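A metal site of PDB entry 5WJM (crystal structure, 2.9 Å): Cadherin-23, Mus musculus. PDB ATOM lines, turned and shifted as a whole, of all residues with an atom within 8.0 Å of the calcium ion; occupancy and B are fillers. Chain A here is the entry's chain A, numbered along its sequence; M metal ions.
The side-chain carboxylate (OD1) of Asp 88 lies within hydrogen-bond range of the backbone NH (N) of Leu 94. The backbone NH (N) of Gly 90 lies within hydrogen-bond range of the side-chain carboxylate (OD1) of Asp 88.
Six residues have an atom within 4 Å of the calcium ion: Asp 2, Asn 3, Asp 33, Asp 35, Asn 39 and Asp 88.
The calcium ion is bound by O of Asn 39, O of Asn 3, OD2 of Asp 88, OD2 of Asp 33, OD1 of Asp 2 and OD2 of Asp 35. Slightly farther from the calcium ion lies OD1 of Asp 33 (2.9 Å).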
ATOM      1  N   ASP A   2     -27.000  -3.216 -15.690  1.00  0.00           N
ATOM      2  CA  ASP A   2     -25.578  -3.485 -16.144  1.00  0.00           C
ATOM      3  C   ASP A   2     -25.531  -4.125 -17.538  1.00  0.00           C
ATOM      4  O   ASP A   2     -26.115  -5.176 -17.756  1.00  0.00           O
ATOM      5  CB  ASP A   2     -24.811  -4.392 -15.149  1.00  0.00           C
ATOM      6  CG  ASP A   2     -23.247  -4.362 -15.358  1.00  0.00           C
ATOM      7  OD1 ASP A   2     -22.756  -3.650 -16.267  1.00  0.00           O
ATOM      8  OD2 ASP A   2     -22.502  -5.039 -14.599  1.00  0.00           O
ATOM      9  N   ASN A   3     -24.791  -3.498 -18.450  1.00  0.00           N
ATOM     10  CA  ASN A   3     -24.508  -4.038 -19.796  1.00  0.00           C
ATOM     11  C   ASN A   3     -23.113  -4.663 -19.828  1.00  0.00           C
ATOM     12  O   ASN A   3     -22.187  -4.154 -19.214  1.00  0.00           O
ATOM     13  CB  ASN A   3     -24.580  -2.938 -20.862  1.00  0.00           C
ATOM     14  CG  ASN A   3     -25.854  -2.108 -20.768  1.00  0.00           C
ATOM     15  OD1 ASN A   3     -26.874  -2.559 -20.233  1.00  0.00           O
ATOM     16  ND2 ASN A   3     -25.791  -0.895 -21.291  1.00  0.00           N
ATOM     17  N   VAL A   4     -22.992  -5.771 -20.566  1.00  0.00           N
ATOM     18  CA  VAL A   4     -21.742  -6.505 -20.691  1.00  0.00           C
ATOM     19  C   VAL A   4     -20.783  -5.682 -21.551  1.00  0.00           C
ATOM     20  O   VAL A   4     -21.211  -5.121 -22.569  1.00  0.00           O
ATOM     21  CB  VAL A   4     -21.968  -7.863 -21.391  1.00  0.00           C
ATOM     22  CG1 VAL A   4     -20.651  -8.594 -21.589  1.00  0.00           C
ATOM     23  CG2 VAL A   4     -22.932  -8.727 -20.592  1.00  0.00           C
ATOM     24  N   PRO A   5     -19.486  -5.590 -21.154  1.00  0.00           N
ATOM     25  CA  PRO A   5     -18.537  -4.954 -22.071  1.00  0.00           C
ATOM     26  C   PRO A   5     -18.270  -5.849 -23.295  1.00  0.00           C
ATOM     27  O   PRO A   5     -17.776  -6.950 -23.119  1.00  0.00           O
ATOM     28  CB  PRO A   5     -17.280  -4.794 -21.224  1.00  0.00           C
ATOM     29  CG  PRO A   5     -17.395  -5.828 -20.172  1.00  0.00           C
ATOM     30  CD  PRO A   5     -18.850  -5.922 -19.867  1.00  0.00           C
ATOM     31  N   THR A   6     -18.603  -5.392 -24.506  1.00  0.00           N
ATOM     32  CA  THR A   6     -18.458  -6.221 -25.719  1.00  0.00           C
ATOM     33  C   THR A   6     -17.314  -5.759 -26.655  1.00  0.00           C
ATOM     34  O   THR A   6     -17.149  -4.556 -26.905  1.00  0.00           O
ATOM     35  CB  THR A   6     -19.775  -6.284 -26.511  1.00  0.00           C
ATOM     36  OG1 THR A   6     -20.265  -4.952 -26.725  1.00  0.00           O
ATOM     37  CG2 THR A   6     -20.836  -7.107 -25.754  1.00  0.00           C
ATOM     38  N   HIS A  32     -16.511  -2.041 -25.727  1.00  0.00           N
ATOM     39  CA  HIS A  32     -17.530  -0.991 -25.594  1.00  0.00           C
ATOM     40  C   HIS A  32     -18.411  -1.263 -24.380  1.00  0.00           C
ATOM     41  O   HIS A  32     -18.868  -2.386 -24.198  1.00  0.00           O
ATOM     42  CB  HIS A  32     -18.395  -0.884 -26.844  1.00  0.00           C
ATOM     43  CG  HIS A  32     -17.684  -0.275 -28.013  1.00  0.00           C
ATOM     44  ND1 HIS A  32     -17.432   1.078 -28.120  1.00  0.00           N
ATOM     45  CD2 HIS A  32     -17.180  -0.841 -29.142  1.00  0.00           C
ATOM     46  CE1 HIS A  32     -16.805   1.328 -29.257  1.00  0.00           C
ATOM     47  NE2 HIS A  32     -16.644   0.173 -29.903  1.00  0.00           N
ATOM     48  N   ASP A  33     -18.620  -0.233 -23.549  1.00  0.00           N
ATOM     49  CA  ASP A  33     -19.415  -0.291 -22.312  1.00  0.00           C
ATOM     50  C   ASP A  33     -19.692   1.155 -21.900  1.00  0.00           C
ATOM     51  O   ASP A  33     -18.814   1.844 -21.356  1.00  0.00           O
ATOM     52  CB  ASP A  33     -18.644  -1.047 -21.200  1.00  0.00           C
ATOM     53  CG  ASP A  33     -19.482  -1.323 -19.938  1.00  0.00           C
ATOM     54  OD1 ASP A  33     -20.411  -0.575 -19.615  1.00  0.00           O
ATOM     55  OD2 ASP A  33     -19.179  -2.306 -19.228  1.00  0.00           O
ATOM     56  N   ARG A  34     -20.920   1.628 -22.177  1.00  0.00           N
ATOM     57  CA  ARG A  34     -21.281   3.017 -21.889  1.00  0.00           C
ATOM     58  C   ARG A  34     -22.094   3.150 -20.588  1.00  0.00           C
ATOM     59  O   ARG A  34     -22.877   4.081 -20.447  1.00  0.00           O
ATOM     60  CB  ARG A  34     -22.021   3.684 -23.078  1.00  0.00           C
ATOM     61  CG  ARG A  34     -21.148   4.012 -24.306  1.00  0.00           C
ATOM     62  CD  ARG A  34     -20.086   5.103 -24.091  1.00  0.00           C
ATOM     63  NE  ARG A  34     -20.623   6.467 -24.222  1.00  0.00           N
ATOM     64  CZ  ARG A  34     -20.784   7.363 -23.229  1.00  0.00           C
ATOM     65  NH1 ARG A  34     -20.439   7.106 -21.967  1.00  0.00           N
ATOM     66  NH2 ARG A  34     -21.304   8.558 -23.515  1.00  0.00           N
ATOM     67  N   ASP A  35     -21.885   2.242 -19.632  1.00  0.00           N
ATOM     68  CA  ASP A  35     -22.543   2.351 -18.330  1.00  0.00           C
ATOM     69  C   ASP A  35     -21.873   3.409 -17.445  1.00  0.00           C
ATOM     70  O   ASP A  35     -20.703   3.767 -17.661  1.00  0.00           O
ATOM     71  CB  ASP A  35     -22.529   1.024 -17.581  1.00  0.00           C
ATOM     72  CG  ASP A  35     -23.315  -0.060 -18.274  1.00  0.00           C
ATOM     73  OD1 ASP A  35     -24.358   0.263 -18.873  1.00  0.00           O
ATOM     74  OD2 ASP A  35     -22.894  -1.239 -18.196  1.00  0.00           O
ATOM     75  N   SER A  36     -22.628   3.865 -16.442  1.00  0.00           N
ATOM     76  CA  SER A  36     -22.163   4.829 -15.425  1.00  0.00           C
ATOM     77  C   SER A  36     -21.454   4.146 -14.260  1.00  0.00           C
ATOM     78  O   SER A  36     -21.754   3.009 -13.877  1.00  0.00           O
ATOM     79  CB  SER A  36     -23.338   5.645 -14.873  1.00  0.00           C
ATOM     80  OG  SER A  36     -23.826   6.551 -15.835  1.00  0.00           O
ATOM     81  N   GLY A  37     -20.497   4.881 -13.691  1.00  0.00           N
ATOM     82  CA  GLY A  37     -19.931   4.540 -12.396  1.00  0.00           C
ATOM     83  C   GLY A  37     -19.128   3.268 -12.448  1.00  0.00           C
ATOM     84  O   GLY A  37     -18.327   3.089 -13.378  1.00  0.00           O
ATOM     85  N   PRO A  38     -19.328   2.380 -11.463  1.00  0.00           N
ATOM     86  CA  PRO A  38     -18.654   1.073 -11.487  1.00  0.00           C
ATOM     87  C   PRO A  38     -19.123   0.091 -12.562  1.00  0.00           C
ATOM     88  O   PRO A  38     -18.374  -0.800 -12.896  1.00  0.00           O
ATOM     89  CB  PRO A  38     -18.937   0.492 -10.107  1.00  0.00           C
ATOM     90  CG  PRO A  38     -19.210   1.669  -9.249  1.00  0.00           C
ATOM     91  CD  PRO A  38     -19.909   2.662 -10.144  1.00  0.00           C
ATOM     92  N   ASN A  39     -20.339   0.229 -13.092  1.00  0.00           N
ATOM     93  CA  ASN A  39     -20.827  -0.740 -14.087  1.00  0.00           C
ATOM     94  C   ASN A  39     -20.195  -0.540 -15.444  1.00  0.00           C
ATOM     95  O   ASN A  39     -20.368  -1.396 -16.314  1.00  0.00           O
ATOM     96  CB  ASN A  39     -22.344  -0.730 -14.223  1.00  0.00           C
ATOM     97  CG  ASN A  39     -23.020  -1.236 -12.971  1.00  0.00           C
ATOM     98  OD1 ASN A  39     -23.275  -2.421 -12.816  1.00  0.00           O
ATOM     99  ND2 ASN A  39     -23.252  -0.326 -12.046  1.00  0.00           N
ATOM    100  N   GLY A  40     -19.511   0.591 -15.633  1.00  0.00           N
ATOM    101  CA  GLY A  40     -18.673   0.821 -16.822  1.00  0.00           C
ATOM    102  C   GLY A  40     -17.197   1.106 -16.529  1.00  0.00           C
ATOM    103  O   GLY A  40     -16.576   1.852 -17.288  1.00  0.00           O
ATOM    104  N   GLN A  41     -16.650   0.561 -15.456  1.00  0.00           N
ATOM    105  CA  GLN A  41     -15.197   0.585 -15.249  1.00  0.00           C
ATOM    106  C   GLN A  41     -14.695  -0.734 -15.768  1.00  0.00           C
ATOM    107  O   GLN A  41     -14.848  -1.761 -15.114  1.00  0.00           O
ATOM    108  CB  GLN A  41     -14.800   0.765 -13.774  1.00  0.00           C
ATOM    109  CG  GLN A  41     -14.842   2.182 -13.237  1.00  0.00           C
ATOM    110  CD  GLN A  41     -14.767   2.223 -11.732  1.00  0.00           C
ATOM    111  OE1 GLN A  41     -14.010   1.468 -11.117  1.00  0.00           O
ATOM    112  NE2 GLN A  41     -15.570   3.100 -11.099  1.00  0.00           N
ATOM    113  N   VAL A  42     -14.103  -0.699 -16.958  1.00  0.00           N
ATOM    114  CA  VAL A  42     -13.608  -1.886 -17.617  1.00  0.00           C
ATOM    115  C   VAL A  42     -12.140  -2.050 -17.256  1.00  0.00           C
ATOM    116  O   VAL A  42     -11.370  -1.087 -17.303  1.00  0.00           O
ATOM    117  CB  VAL A  42     -13.798  -1.761 -19.128  1.00  0.00           C
ATOM    118  CG1 VAL A  42     -13.202  -2.949 -19.848  1.00  0.00           C
ATOM    119  CG2 VAL A  42     -15.290  -1.630 -19.429  1.00  0.00           C
ATOM    120  N   ARG A  87     -13.474  -6.999 -18.047  1.00  0.00           N
ATOM    121  CA  ARG A  87     -14.463  -7.164 -16.973  1.00  0.00           C
ATOM    122  C   ARG A  87     -14.821  -5.813 -16.399  1.00  0.00           C
ATOM    123  O   ARG A  87     -13.919  -5.005 -16.183  1.00  0.00           O
ATOM    124  CB  ARG A  87     -13.959  -8.094 -15.851  1.00  0.00           C
ATOM    125  CG  ARG A  87     -13.203  -7.433 -14.680  1.00  0.00           C
ATOM    126  CD  ARG A  87     -12.752  -8.436 -13.607  1.00  0.00           C
ATOM    127  NE  ARG A  87     -13.849  -9.368 -13.247  1.00  0.00           N
ATOM    128  CZ  ARG A  87     -14.024 -10.605 -13.734  1.00  0.00           C
ATOM    129  NH1 ARG A  87     -13.178 -11.152 -14.615  1.00  0.00           N
ATOM    130  NH2 ARG A  87     -15.074 -11.329 -13.315  1.00  0.00           N
ATOM    131  N   ASP A  88     -16.120  -5.585 -16.132  1.00  0.00           N
ATOM    132  CA  ASP A  88     -16.577  -4.382 -15.414  1.00  0.00           C
ATOM    133  C   ASP A  88     -16.563  -4.625 -13.912  1.00  0.00           C
ATOM    134  O   ASP A  88     -16.262  -5.738 -13.467  1.00  0.00           O
ATOM    135  CB  ASP A  88     -17.927  -3.783 -15.950  1.00  0.00           C
ATOM    136  CG  ASP A  88     -19.176  -4.711 -15.777  1.00  0.00           C
ATOM    137  OD1 ASP A  88     -19.224  -5.599 -14.896  1.00  0.00           O
ATOM    138  OD2 ASP A  88     -20.148  -4.512 -16.528  1.00  0.00           O
ATOM    139  N   ARG A  89     -16.826  -3.571 -13.140  1.00  0.00           N
ATOM    140  CA  ARG A  89     -16.923  -3.640 -11.677  1.00  0.00           C
ATOM    141  C   ARG A  89     -18.363  -3.581 -11.141  1.00  0.00           C
ATOM    142  O   ARG A  89     -18.614  -3.007 -10.069  1.00  0.00           O
ATOM    143  CB  ARG A  89     -16.065  -2.563 -11.045  1.00  0.00           C
ATOM    144  CG  ARG A  89     -14.587  -2.732 -11.296  1.00  0.00           C
ATOM    145  CD  ARG A  89     -13.842  -1.463 -10.944  1.00  0.00           C
ATOM    146  NE  ARG A  89     -12.510  -1.740 -10.434  1.00  0.00           N
ATOM    147  CZ  ARG A  89     -12.235  -2.277  -9.238  1.00  0.00           C
ATOM    148  NH1 ARG A  89     -13.213  -2.583  -8.381  1.00  0.00           N
ATOM    149  NH2 ARG A  89     -10.969  -2.501  -8.898  1.00  0.00           N
ATOM    150  N   GLY A  90     -19.295  -4.208 -11.868  1.00  0.00           N
ATOM    151  CA  GLY A  90     -20.680  -4.372 -11.431  1.00  0.00           C
ATOM    152  C   GLY A  90     -20.824  -5.609 -10.566  1.00  0.00           C
ATOM    153  O   GLY A  90     -19.855  -6.336 -10.353  1.00  0.00           O
ATOM    154  N   PRO A  92     -23.406  -8.887 -10.161  1.00  0.00           N
ATOM    155  CA  PRO A  92     -22.111  -9.547 -10.464  1.00  0.00           C
ATOM    156  C   PRO A  92     -21.300  -8.847 -11.591  1.00  0.00           C
ATOM    157  O   PRO A  92     -21.869  -8.104 -12.405  1.00  0.00           O
ATOM    158  CB  PRO A  92     -22.533 -10.953 -10.893  1.00  0.00           C
ATOM    159  CG  PRO A  92     -23.962 -10.805 -11.393  1.00  0.00           C
ATOM    160  CD  PRO A  92     -24.540  -9.496 -10.873  1.00  0.00           C
ATOM    161  N   PRO A  93     -19.964  -9.041 -11.598  1.00  0.00           N
ATOM    162  CA  PRO A  93     -19.182  -8.461 -12.667  1.00  0.00           C
ATOM    163  C   PRO A  93     -19.393  -9.198 -13.978  1.00  0.00           C
ATOM    164  O   PRO A  93     -19.273 -10.431 -14.047  1.00  0.00           O
ATOM    165  CB  PRO A  93     -17.737  -8.609 -12.181  1.00  0.00           C
ATOM    166  CG  PRO A  93     -17.781  -9.677 -11.164  1.00  0.00           C
ATOM    167  CD  PRO A  93     -19.119  -9.560 -10.517  1.00  0.00           C
ATOM    168  N   LEU A  94     -19.727  -8.435 -15.018  1.00  0.00           N
ATOM    169  CA  LEU A  94     -19.924  -8.972 -16.349  1.00  0.00           C
ATOM    170  C   LEU A  94     -18.630  -8.895 -17.157  1.00  0.00           C
ATOM    171  O   LEU A  94     -17.791  -8.009 -16.931  1.00  0.00           O
ATOM    172  CB  LEU A  94     -21.030  -8.193 -17.043  1.00  0.00           C
ATOM    173  CG  LEU A  94     -22.347  -8.160 -16.285  1.00  0.00           C
ATOM    174  CD1 LEU A  94     -23.379  -7.466 -17.147  1.00  0.00           C
ATOM    175  CD2 LEU A  94     -22.794  -9.576 -15.888  1.00  0.00           C
ATOM    176  N   SER A  95     -18.469  -9.822 -18.097  1.00  0.00           N
ATOM    177  CA  SER A  95     -17.246  -9.861 -18.881  1.00  0.00           C
ATOM    178  C   SER A  95     -17.414 -10.544 -20.223  1.00  0.00           C
ATOM    179  O   SER A  95     -18.360 -11.304 -20.460  1.00  0.00           O
ATOM    180  CB  SER A  95     -16.145 -10.528 -18.089  1.00  0.00           C
ATOM    181  OG  SER A  95     -16.538 -11.813 -17.720  1.00  0.00           O
HETATM  182 CA    CA M   1     -21.006  -2.800 -17.797  1.00  0.00          CA
